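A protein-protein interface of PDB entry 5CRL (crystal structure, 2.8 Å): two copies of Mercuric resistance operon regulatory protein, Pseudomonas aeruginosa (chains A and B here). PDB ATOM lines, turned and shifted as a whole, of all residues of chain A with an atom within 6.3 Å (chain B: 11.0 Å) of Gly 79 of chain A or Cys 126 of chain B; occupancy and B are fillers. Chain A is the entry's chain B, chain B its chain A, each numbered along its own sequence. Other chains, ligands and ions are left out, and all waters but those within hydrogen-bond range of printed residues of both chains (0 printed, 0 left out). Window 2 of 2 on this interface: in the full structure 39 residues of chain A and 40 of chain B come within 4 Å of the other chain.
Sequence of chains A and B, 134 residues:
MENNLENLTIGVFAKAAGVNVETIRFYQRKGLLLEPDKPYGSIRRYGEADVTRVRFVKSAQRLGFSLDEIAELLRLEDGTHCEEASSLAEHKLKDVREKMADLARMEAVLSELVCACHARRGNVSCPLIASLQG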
ATOM      1  N   LEU A  76      -0.308   6.020   9.910  1.00  0.00           N
ATOM      2  CA  LEU A  76      -0.054   4.626   9.562  1.00  0.00           C
ATOM      3  C   LEU A  76       1.432   4.359   9.283  1.00  0.00           C
ATOM      4  O   LEU A  76       1.757   3.378   8.620  1.00  0.00           O
ATOM      5  CB  LEU A  76      -0.893   4.248   8.330  1.00  0.00           C
ATOM      6  CG  LEU A  76      -2.320   4.826   8.279  1.00  0.00           C
ATOM      7  CD1 LEU A  76      -3.033   4.408   7.003  1.00  0.00           C
ATOM      8  CD2 LEU A  76      -3.133   4.416   9.501  1.00  0.00           C
ATOM      9  N   GLU A  77       2.320   5.209   9.807  1.00  0.00           N
ATOM     10  CA  GLU A  77       3.766   5.156   9.520  1.00  0.00           C
ATOM     11  C   GLU A  77       4.483   3.861   9.943  1.00  0.00           C
ATOM     12  O   GLU A  77       5.524   3.523   9.379  1.00  0.00           O
ATOM     13  CB  GLU A  77       4.466   6.374  10.151  1.00  0.00           C
ATOM     14  CG  GLU A  77       5.935   6.553   9.788  1.00  0.00           C
ATOM     15  CD  GLU A  77       6.492   7.905  10.223  1.00  0.00           C
ATOM     16  OE1 GLU A  77       5.950   8.491  11.194  1.00  0.00           O
ATOM     17  OE2 GLU A  77       7.474   8.392   9.598  1.00  0.00           O
ATOM     18  N   ASP A  78       3.941   3.134  10.921  1.00  0.00           N
ATOM     19  CA  ASP A  78       4.570   1.883  11.382  1.00  0.00           C
ATOM     20  C   ASP A  78       4.349   0.670  10.450  1.00  0.00           C
ATOM     21  O   ASP A  78       4.887  -0.409  10.689  1.00  0.00           O
ATOM     22  CB  ASP A  78       4.139   1.547  12.818  1.00  0.00           C
ATOM     23  CG  ASP A  78       2.690   1.099  12.917  1.00  0.00           C
ATOM     24  OD1 ASP A  78       2.013   0.995  11.879  1.00  0.00           O
ATOM     25  OD2 ASP A  78       2.230   0.847  14.050  1.00  0.00           O
ATOM     26  N   GLY A  79       3.537   0.844   9.413  1.00  0.00           N
ATOM     27  CA  GLY A  79       3.460  -0.127   8.317  1.00  0.00           C
ATOM     28  C   GLY A  79       2.746  -1.426   8.633  1.00  0.00           C
ATOM     29  O   GLY A  79       3.124  -2.487   8.133  1.00  0.00           O
ATOM     30  N   THR A  80       1.708  -1.341   9.455  1.00  0.00           N
ATOM     31  CA  THR A  80       0.937  -2.513   9.846  1.00  0.00           C
ATOM     32  C   THR A  80      -0.557  -2.270   9.632  1.00  0.00           C
ATOM     33  O   THR A  80      -1.387  -2.902  10.274  1.00  0.00           O
ATOM     34  CB  THR A  80       1.203  -2.857  11.325  1.00  0.00           C
ATOM     35  OG1 THR A  80       0.667  -1.822  12.156  1.00  0.00           O
ATOM     36  CG2 THR A  80       2.710  -2.992  11.593  1.00  0.00           C
ATOM     37  N   HIS A  81      -0.890  -1.343   8.730  1.00  0.00           N
ATOM     38  CA  HIS A  81      -2.284  -1.006   8.411  1.00  0.00           C
ATOM     39  C   HIS A  81      -2.462  -0.887   6.896  1.00  0.00           C
ATOM     40  O   HIS A  81      -2.830   0.168   6.380  1.00  0.00           O
ATOM     41  CB  HIS A  81      -2.699   0.312   9.083  1.00  0.00           C
ATOM     42  CG  HIS A  81      -2.606   0.297  10.579  1.00  0.00           C
ATOM     43  ND1 HIS A  81      -1.875   1.226  11.289  1.00  0.00           N
ATOM     44  CD2 HIS A  81      -3.169  -0.522  11.500  1.00  0.00           C
ATOM     45  CE1 HIS A  81      -1.989   0.978  12.581  1.00  0.00           C
ATOM     46  NE2 HIS A  81      -2.767  -0.078  12.736  1.00  0.00           N
ATOM     47  N   CYS A  82      -2.203  -1.984   6.195  1.00  0.00           N
ATOM     48  CA  CYS A  82      -2.248  -2.016   4.732  1.00  0.00           C
ATOM     49  C   CYS A  82      -3.625  -1.667   4.147  1.00  0.00           C
ATOM     50  O   CYS A  82      -3.717  -0.910   3.180  1.00  0.00           O
ATOM     51  CB  CYS A  82      -1.809  -3.394   4.231  1.00  0.00           C
ATOM     52  SG  CYS A  82      -1.536  -3.482   2.450  1.00  0.00           S
ATOM     53  N   ALA A  85      -4.072   1.994   4.278  1.00  0.00           N
ATOM     54  CA  ALA A  85      -3.119   2.715   3.428  1.00  0.00           C
ATOM     55  C   ALA A  85      -3.593   2.733   1.989  1.00  0.00           C
ATOM     56  O   ALA A  85      -3.720   3.801   1.390  1.00  0.00           O
ATOM     57  CB  ALA A  85      -1.746   2.084   3.515  1.00  0.00           C
ATOM     58  N   SER A  86      -3.877   1.545   1.461  1.00  0.00           N
ATOM     59  CA  SER A  86      -4.415   1.397   0.106  1.00  0.00           C
ATOM     60  C   SER A  86      -5.572   2.351  -0.128  1.00  0.00           C
ATOM     61  O   SER A  86      -5.644   3.014  -1.162  1.00  0.00           O
ATOM     62  CB  SER A  86      -4.914  -0.028  -0.145  1.00  0.00           C
ATOM     63  OG  SER A  86      -4.185  -0.963   0.620  1.00  0.00           O
ATOM     64  N   GLU B 112       0.728   1.528  -9.430  1.00  0.00           N
ATOM     65  CA  GLU B 112       1.769   0.542  -9.162  1.00  0.00           C
ATOM     66  C   GLU B 112       1.818   0.203  -7.677  1.00  0.00           C
ATOM     67  O   GLU B 112       1.955  -0.960  -7.303  1.00  0.00           O
ATOM     68  CB  GLU B 112       3.098   1.123  -9.612  1.00  0.00           C
ATOM     69  CG  GLU B 112       4.218   0.142  -9.828  1.00  0.00           C
ATOM     70  CD  GLU B 112       5.380   0.799 -10.552  1.00  0.00           C
ATOM     71  OE1 GLU B 112       5.903   0.180 -11.504  1.00  0.00           O
ATOM     72  OE2 GLU B 112       5.753   1.931 -10.169  1.00  0.00           O
ATOM     73  N   LEU B 113       1.668   1.219  -6.832  1.00  0.00           N
ATOM     74  CA  LEU B 113       1.659   1.005  -5.386  1.00  0.00           C
ATOM     75  C   LEU B 113       0.439   0.183  -4.964  1.00  0.00           C
ATOM     76  O   LEU B 113       0.570  -0.802  -4.246  1.00  0.00           O
ATOM     77  CB  LEU B 113       1.702   2.342  -4.625  1.00  0.00           C
ATOM     78  CG  LEU B 113       2.969   3.188  -4.844  1.00  0.00           C
ATOM     79  CD1 LEU B 113       2.763   4.613  -4.356  1.00  0.00           C
ATOM     80  CD2 LEU B 113       4.201   2.563  -4.197  1.00  0.00           C
ATOM     81  N   VAL B 114      -0.738   0.579  -5.431  1.00  0.00           N
ATOM     82  CA  VAL B 114      -1.964  -0.140  -5.111  1.00  0.00           C
ATOM     83  C   VAL B 114      -1.858  -1.607  -5.528  1.00  0.00           C
ATOM     84  O   VAL B 114      -2.135  -2.506  -4.740  1.00  0.00           O
ATOM     85  CB  VAL B 114      -3.184   0.503  -5.804  1.00  0.00           C
ATOM     86  CG1 VAL B 114      -4.401  -0.408  -5.719  1.00  0.00           C
ATOM     87  CG2 VAL B 114      -3.489   1.862  -5.184  1.00  0.00           C
ATOM     88  N   CYS B 115      -1.472  -1.841  -6.776  1.00  0.00           N
ATOM     89  CA  CYS B 115      -1.239  -3.196  -7.277  1.00  0.00           C
ATOM     90  C   CYS B 115      -0.423  -4.015  -6.258  1.00  0.00           C
ATOM     91  O   CYS B 115      -0.801  -5.127  -5.893  1.00  0.00           O
ATOM     92  CB  CYS B 115      -0.542  -3.121  -8.648  1.00  0.00           C
ATOM     93  SG  CYS B 115       0.200  -4.649  -9.273  1.00  0.00           S
ATOM     94  N   ALA B 116       0.665  -3.432  -5.763  1.00  0.00           N
ATOM     95  CA  ALA B 116       1.515  -4.108  -4.793  1.00  0.00           C
ATOM     96  C   ALA B 116       0.874  -4.198  -3.415  1.00  0.00           C
ATOM     97  O   ALA B 116       1.160  -5.123  -2.668  1.00  0.00           O
ATOM     98  CB  ALA B 116       2.856  -3.409  -4.695  1.00  0.00           C
ATOM     99  N   CYS B 117       0.033  -3.235  -3.060  1.00  0.00           N
ATOM    100  CA  CYS B 117      -0.714  -3.314  -1.804  1.00  0.00           C
ATOM    101  C   CYS B 117      -1.604  -4.566  -1.800  1.00  0.00           C
ATOM    102  O   CYS B 117      -1.508  -5.408  -0.901  1.00  0.00           O
ATOM    103  CB  CYS B 117      -1.578  -2.060  -1.576  1.00  0.00           C
ATOM    104  SG  CYS B 117      -0.753  -0.659  -0.771  1.00  0.00           S
ATOM    105  N   HIS B 118      -2.456  -4.685  -2.820  1.00  0.00           N
ATOM    106  CA  HIS B 118      -3.403  -5.806  -2.936  1.00  0.00           C
ATOM    107  C   HIS B 118      -2.699  -7.163  -3.034  1.00  0.00           C
ATOM    108  O   HIS B 118      -3.222  -8.178  -2.570  1.00  0.00           O
ATOM    109  CB  HIS B 118      -4.316  -5.637  -4.164  1.00  0.00           C
ATOM    110  CG  HIS B 118      -5.207  -4.428  -4.117  1.00  0.00           C
ATOM    111  ND1 HIS B 118      -5.608  -3.831  -2.938  1.00  0.00           N
ATOM    112  CD2 HIS B 118      -5.806  -3.729  -5.111  1.00  0.00           C
ATOM    113  CE1 HIS B 118      -6.393  -2.805  -3.209  1.00  0.00           C
ATOM    114  NE2 HIS B 118      -6.533  -2.723  -4.521  1.00  0.00           N
ATOM    115  N   ALA B 119      -1.503  -7.169  -3.618  1.00  0.00           N
ATOM    116  CA  ALA B 119      -0.772  -8.403  -3.859  1.00  0.00           C
ATOM    117  C   ALA B 119       0.046  -8.891  -2.652  1.00  0.00           C
ATOM    118  O   ALA B 119       0.777  -9.873  -2.768  1.00  0.00           O
ATOM    119  CB  ALA B 119       0.120  -8.231  -5.076  1.00  0.00           C
ATOM    120  N   ARG B 120      -0.078  -8.230  -1.499  1.00  0.00           N
ATOM    121  CA  ARG B 120       0.641  -8.651  -0.295  1.00  0.00           C
ATOM    122  C   ARG B 120      -0.024  -9.876   0.317  1.00  0.00           C
ATOM    123  O   ARG B 120       0.592 -10.936   0.422  1.00  0.00           O
ATOM    124  CB  ARG B 120       0.708  -7.518   0.724  1.00  0.00           C
ATOM    125  N   CYS B 126       3.610  -3.129   4.846  1.00  0.00           N
ATOM    126  CA  CYS B 126       2.853  -2.365   3.867  1.00  0.00           C
ATOM    127  C   CYS B 126       3.779  -1.771   2.806  1.00  0.00           C
ATOM    128  O   CYS B 126       4.621  -0.917   3.127  1.00  0.00           O
ATOM    129  CB  CYS B 126       2.067  -1.239   4.534  1.00  0.00           C
ATOM    130  SG  CYS B 126       1.170  -0.188   3.352  1.00  0.00           S
ATOM    131  N   PRO B 127       3.635  -2.219   1.545  1.00  0.00           N
ATOM    132  CA  PRO B 127       4.488  -1.744   0.453  1.00  0.00           C
ATOM    133  C   PRO B 127       4.379  -0.246   0.195  1.00  0.00           C
ATOM    134  O   PRO B 127       5.361   0.377  -0.208  1.00  0.00           O
ATOM    135  CB  PRO B 127       3.969  -2.518  -0.761  1.00  0.00           C
ATOM    136  CG  PRO B 127       3.346  -3.744  -0.199  1.00  0.00           C
ATOM    137  CD  PRO B 127       2.758  -3.319   1.110  1.00  0.00           C
ATOM    138  N   LEU B 128       3.200   0.324   0.416  1.00  0.00           N
ATOM    139  CA  LEU B 128       2.993   1.750   0.186  1.00  0.00           C
ATOM    140  C   LEU B 128       3.927   2.547   1.081  1.00  0.00           C
ATOM    141  O   LEU B 128       4.714   3.362   0.601  1.00  0.00           O
ATOM    142  CB  LEU B 128       1.542   2.135   0.457  1.00  0.00           C
ATOM    143  CG  LEU B 128       1.060   3.452  -0.151  1.00  0.00           C
ATOM    144  CD1 LEU B 128      -0.438   3.379  -0.416  1.00  0.00           C
ATOM    145  CD2 LEU B 128       1.395   4.630   0.742  1.00  0.00           C
ATOM    146  N   ILE B 129       3.847   2.284   2.380  1.00  0.00           N
ATOM    147  CA  ILE B 129       4.720   2.916   3.363  1.00  0.00           C
ATOM    148  C   ILE B 129       6.175   2.593   3.057  1.00  0.00           C
ATOM    149  O   ILE B 129       7.018   3.482   3.038  1.00  0.00           O
ATOM    150  CB  ILE B 129       4.393   2.439   4.789  1.00  0.00           C
ATOM    151  CG1 ILE B 129       3.242   3.252   5.399  1.00  0.00           C
ATOM    152  CG2 ILE B 129       5.606   2.597   5.694  1.00  0.00           C
ATOM    153  CD1 ILE B 129       2.061   3.511   4.489  1.00  0.00           C
ATOM    154  N   ALA B 130       6.459   1.319   2.811  1.00  0.00           N
ATOM    155  CA  ALA B 130       7.813   0.897   2.469  1.00  0.00           C
ATOM    156  C   ALA B 130       8.374   1.762   1.344  1.00  0.00           C
ATOM    157  O   ALA B 130       9.456   2.333   1.488  1.00  0.00           O
ATOM    158  CB  ALA B 130       7.833  -0.566   2.066  1.00  0.00           C
ATOM    159  N   SER B 131       7.622   1.871   0.248  1.00  0.00           N
ATOM    160  CA  SER B 131       8.018   2.703  -0.896  1.00  0.00           C
ATOM    161  C   SER B 131       8.153   4.186  -0.548  1.00  0.00           C
ATOM    162  O   SER B 131       9.006   4.880  -1.114  1.00  0.00           O
ATOM    163  CB  SER B 131       7.053   2.531  -2.080  1.00  0.00           C
ATOM    164  OG  SER B 131       7.541   1.548  -2.985  1.00  0.00           O
ATOM    165  N   LEU B 132       7.328   4.668   0.379  1.00  0.00           N
ATOM    166  CA  LEU B 132       7.426   6.063   0.831  1.00  0.00           C
ATOM    167  C   LEU B 132       8.645   6.323   1.718  1.00  0.00           C
ATOM    168  O   LEU B 132       9.013   7.483   1.940  1.00  0.00           O
ATOM    169  CB  LEU B 132       6.156   6.498   1.553  1.00  0.00           C
ATOM    170  CG  LEU B 132       5.068   7.087   0.656  1.00  0.00           C
ATOM    171  CD1 LEU B 132       4.882   6.324  -0.652  1.00  0.00           C
ATOM    172  CD2 LEU B 132       3.763   7.170   1.435  1.00  0.00           C
ATOM    173  N   GLN B 133       9.271   5.252   2.206  1.00  0.00           N
ATOM    174  CA  GLN B 133      10.459   5.354   3.043  1.00  0.00           C
ATOM    175  C   GLN B 133      11.700   4.885   2.295  1.00  0.00           C
ATOM    176  O   GLN B 133      12.188   5.581   1.415  1.00  0.00           O
ATOM    177  CB  GLN B 133      10.274   4.512   4.295  1.00  0.00           C
ATOM    178  CG  GLN B 133       9.115   4.973   5.162  1.00  0.00           C
ATOM    179  CD  GLN B 133       8.826   4.036   6.318  1.00  0.00           C
ATOM    180  OE1 GLN B 133       9.188   2.856   6.283  1.00  0.00           O
ATOM    181  NE2 GLN B 133       8.165   4.556   7.354  1.00  0.00           N
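O of Glu 77 of chain A sits at hydrogen-bond distance from NE2 of Gln 133 of chain B.
N of Cys 126 of chain B sits at hydrogen-bond distance from O of Gly 79 of chain A.
SG of Cys 117 of chain B lies close to OG of Ser 86 of chain A (3.7 Å).
The side-chain sulfur of Cys 126 of chain B sits close to the backbone NH of Leu 128 of chain B (3.6 Å).
O of Cys 82 of chain A sits at hydrogen-bond distance from OG of Ser 86 of chain A (2.6 Å).
The side-chain sulfur (SG) of Cys 117 of chain B sits close to the backbone carbonyl oxygen (O) of Leu 113 of chain B, 3.7 Å away.
SG of Cys 126 of chain B sits close to N of Ile 129 of chain B, at 3.8 Å.
Ile 129 of chain B touches Leu 76 of chain A.
O of Glu 77 of chain A touches CG2 of Ile 129 of chain B (3.8 Å).
SG of Cys 82 of chain A touches O of Cys 117 of chain B, 3.9 Å away.
Cys 126 of chain B touches Ala 85 of chain A.
Leu 128 of chain B touches Ala 85 of chain A (CD1 to O, 3.8 Å).
Of chain B, only Cys 126 comes within 4 Å of Gly 79 of chain A.
Cys 126 of chain B touches just these residues of chain A: Gly 79 and Ala 85.
No residue of chain B comes within 4 Å of Thr 80 of chain A.
Of chain B, only Cys 117 (3.9 Å) comes within 4 Å of Cys 82 of chain A.
Of chain B, only Cys 126 (3.7 Å) and Leu 128 (3.8 Å) come within 4 Å of Ala 85 of chain A.
Of the printed residues of chain B, Leu 76 of chain A touches Ile 129 (3.5 Å).
Of the printed residues of chain A, Ile 129 of chain B touches Leu 76 (3.5 Å) and Glu 77 (3.8 Å).
Leu 132 of chain B touches none of the printed residues of chain A.
Arg 120 of chain B touches none of the printed residues of chain A.
The nearest residue of chain A that does not touch Cys 126 of chain B is Cys 82 of chain A (4.1 Å).
Of the 9 printed residues of chain A, 6 touch a printed residue of chain B.
Hydrophobic or aromatic side chains of chain A within 4 Å of the printed part of chain B: Ala 85.
Of the 17 printed residues of chain B, 5 touch a printed residue of chain A.
Printed residues of chain B that touch a printed residue of chain A: Cys 117, Cys 126, Leu 128, Ile 129 and Gln 133.
Hydrophobic or aromatic side chains of chain B that line the printed part of chain A: Leu 128 and Ile 129.
No position is printed for both chains.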
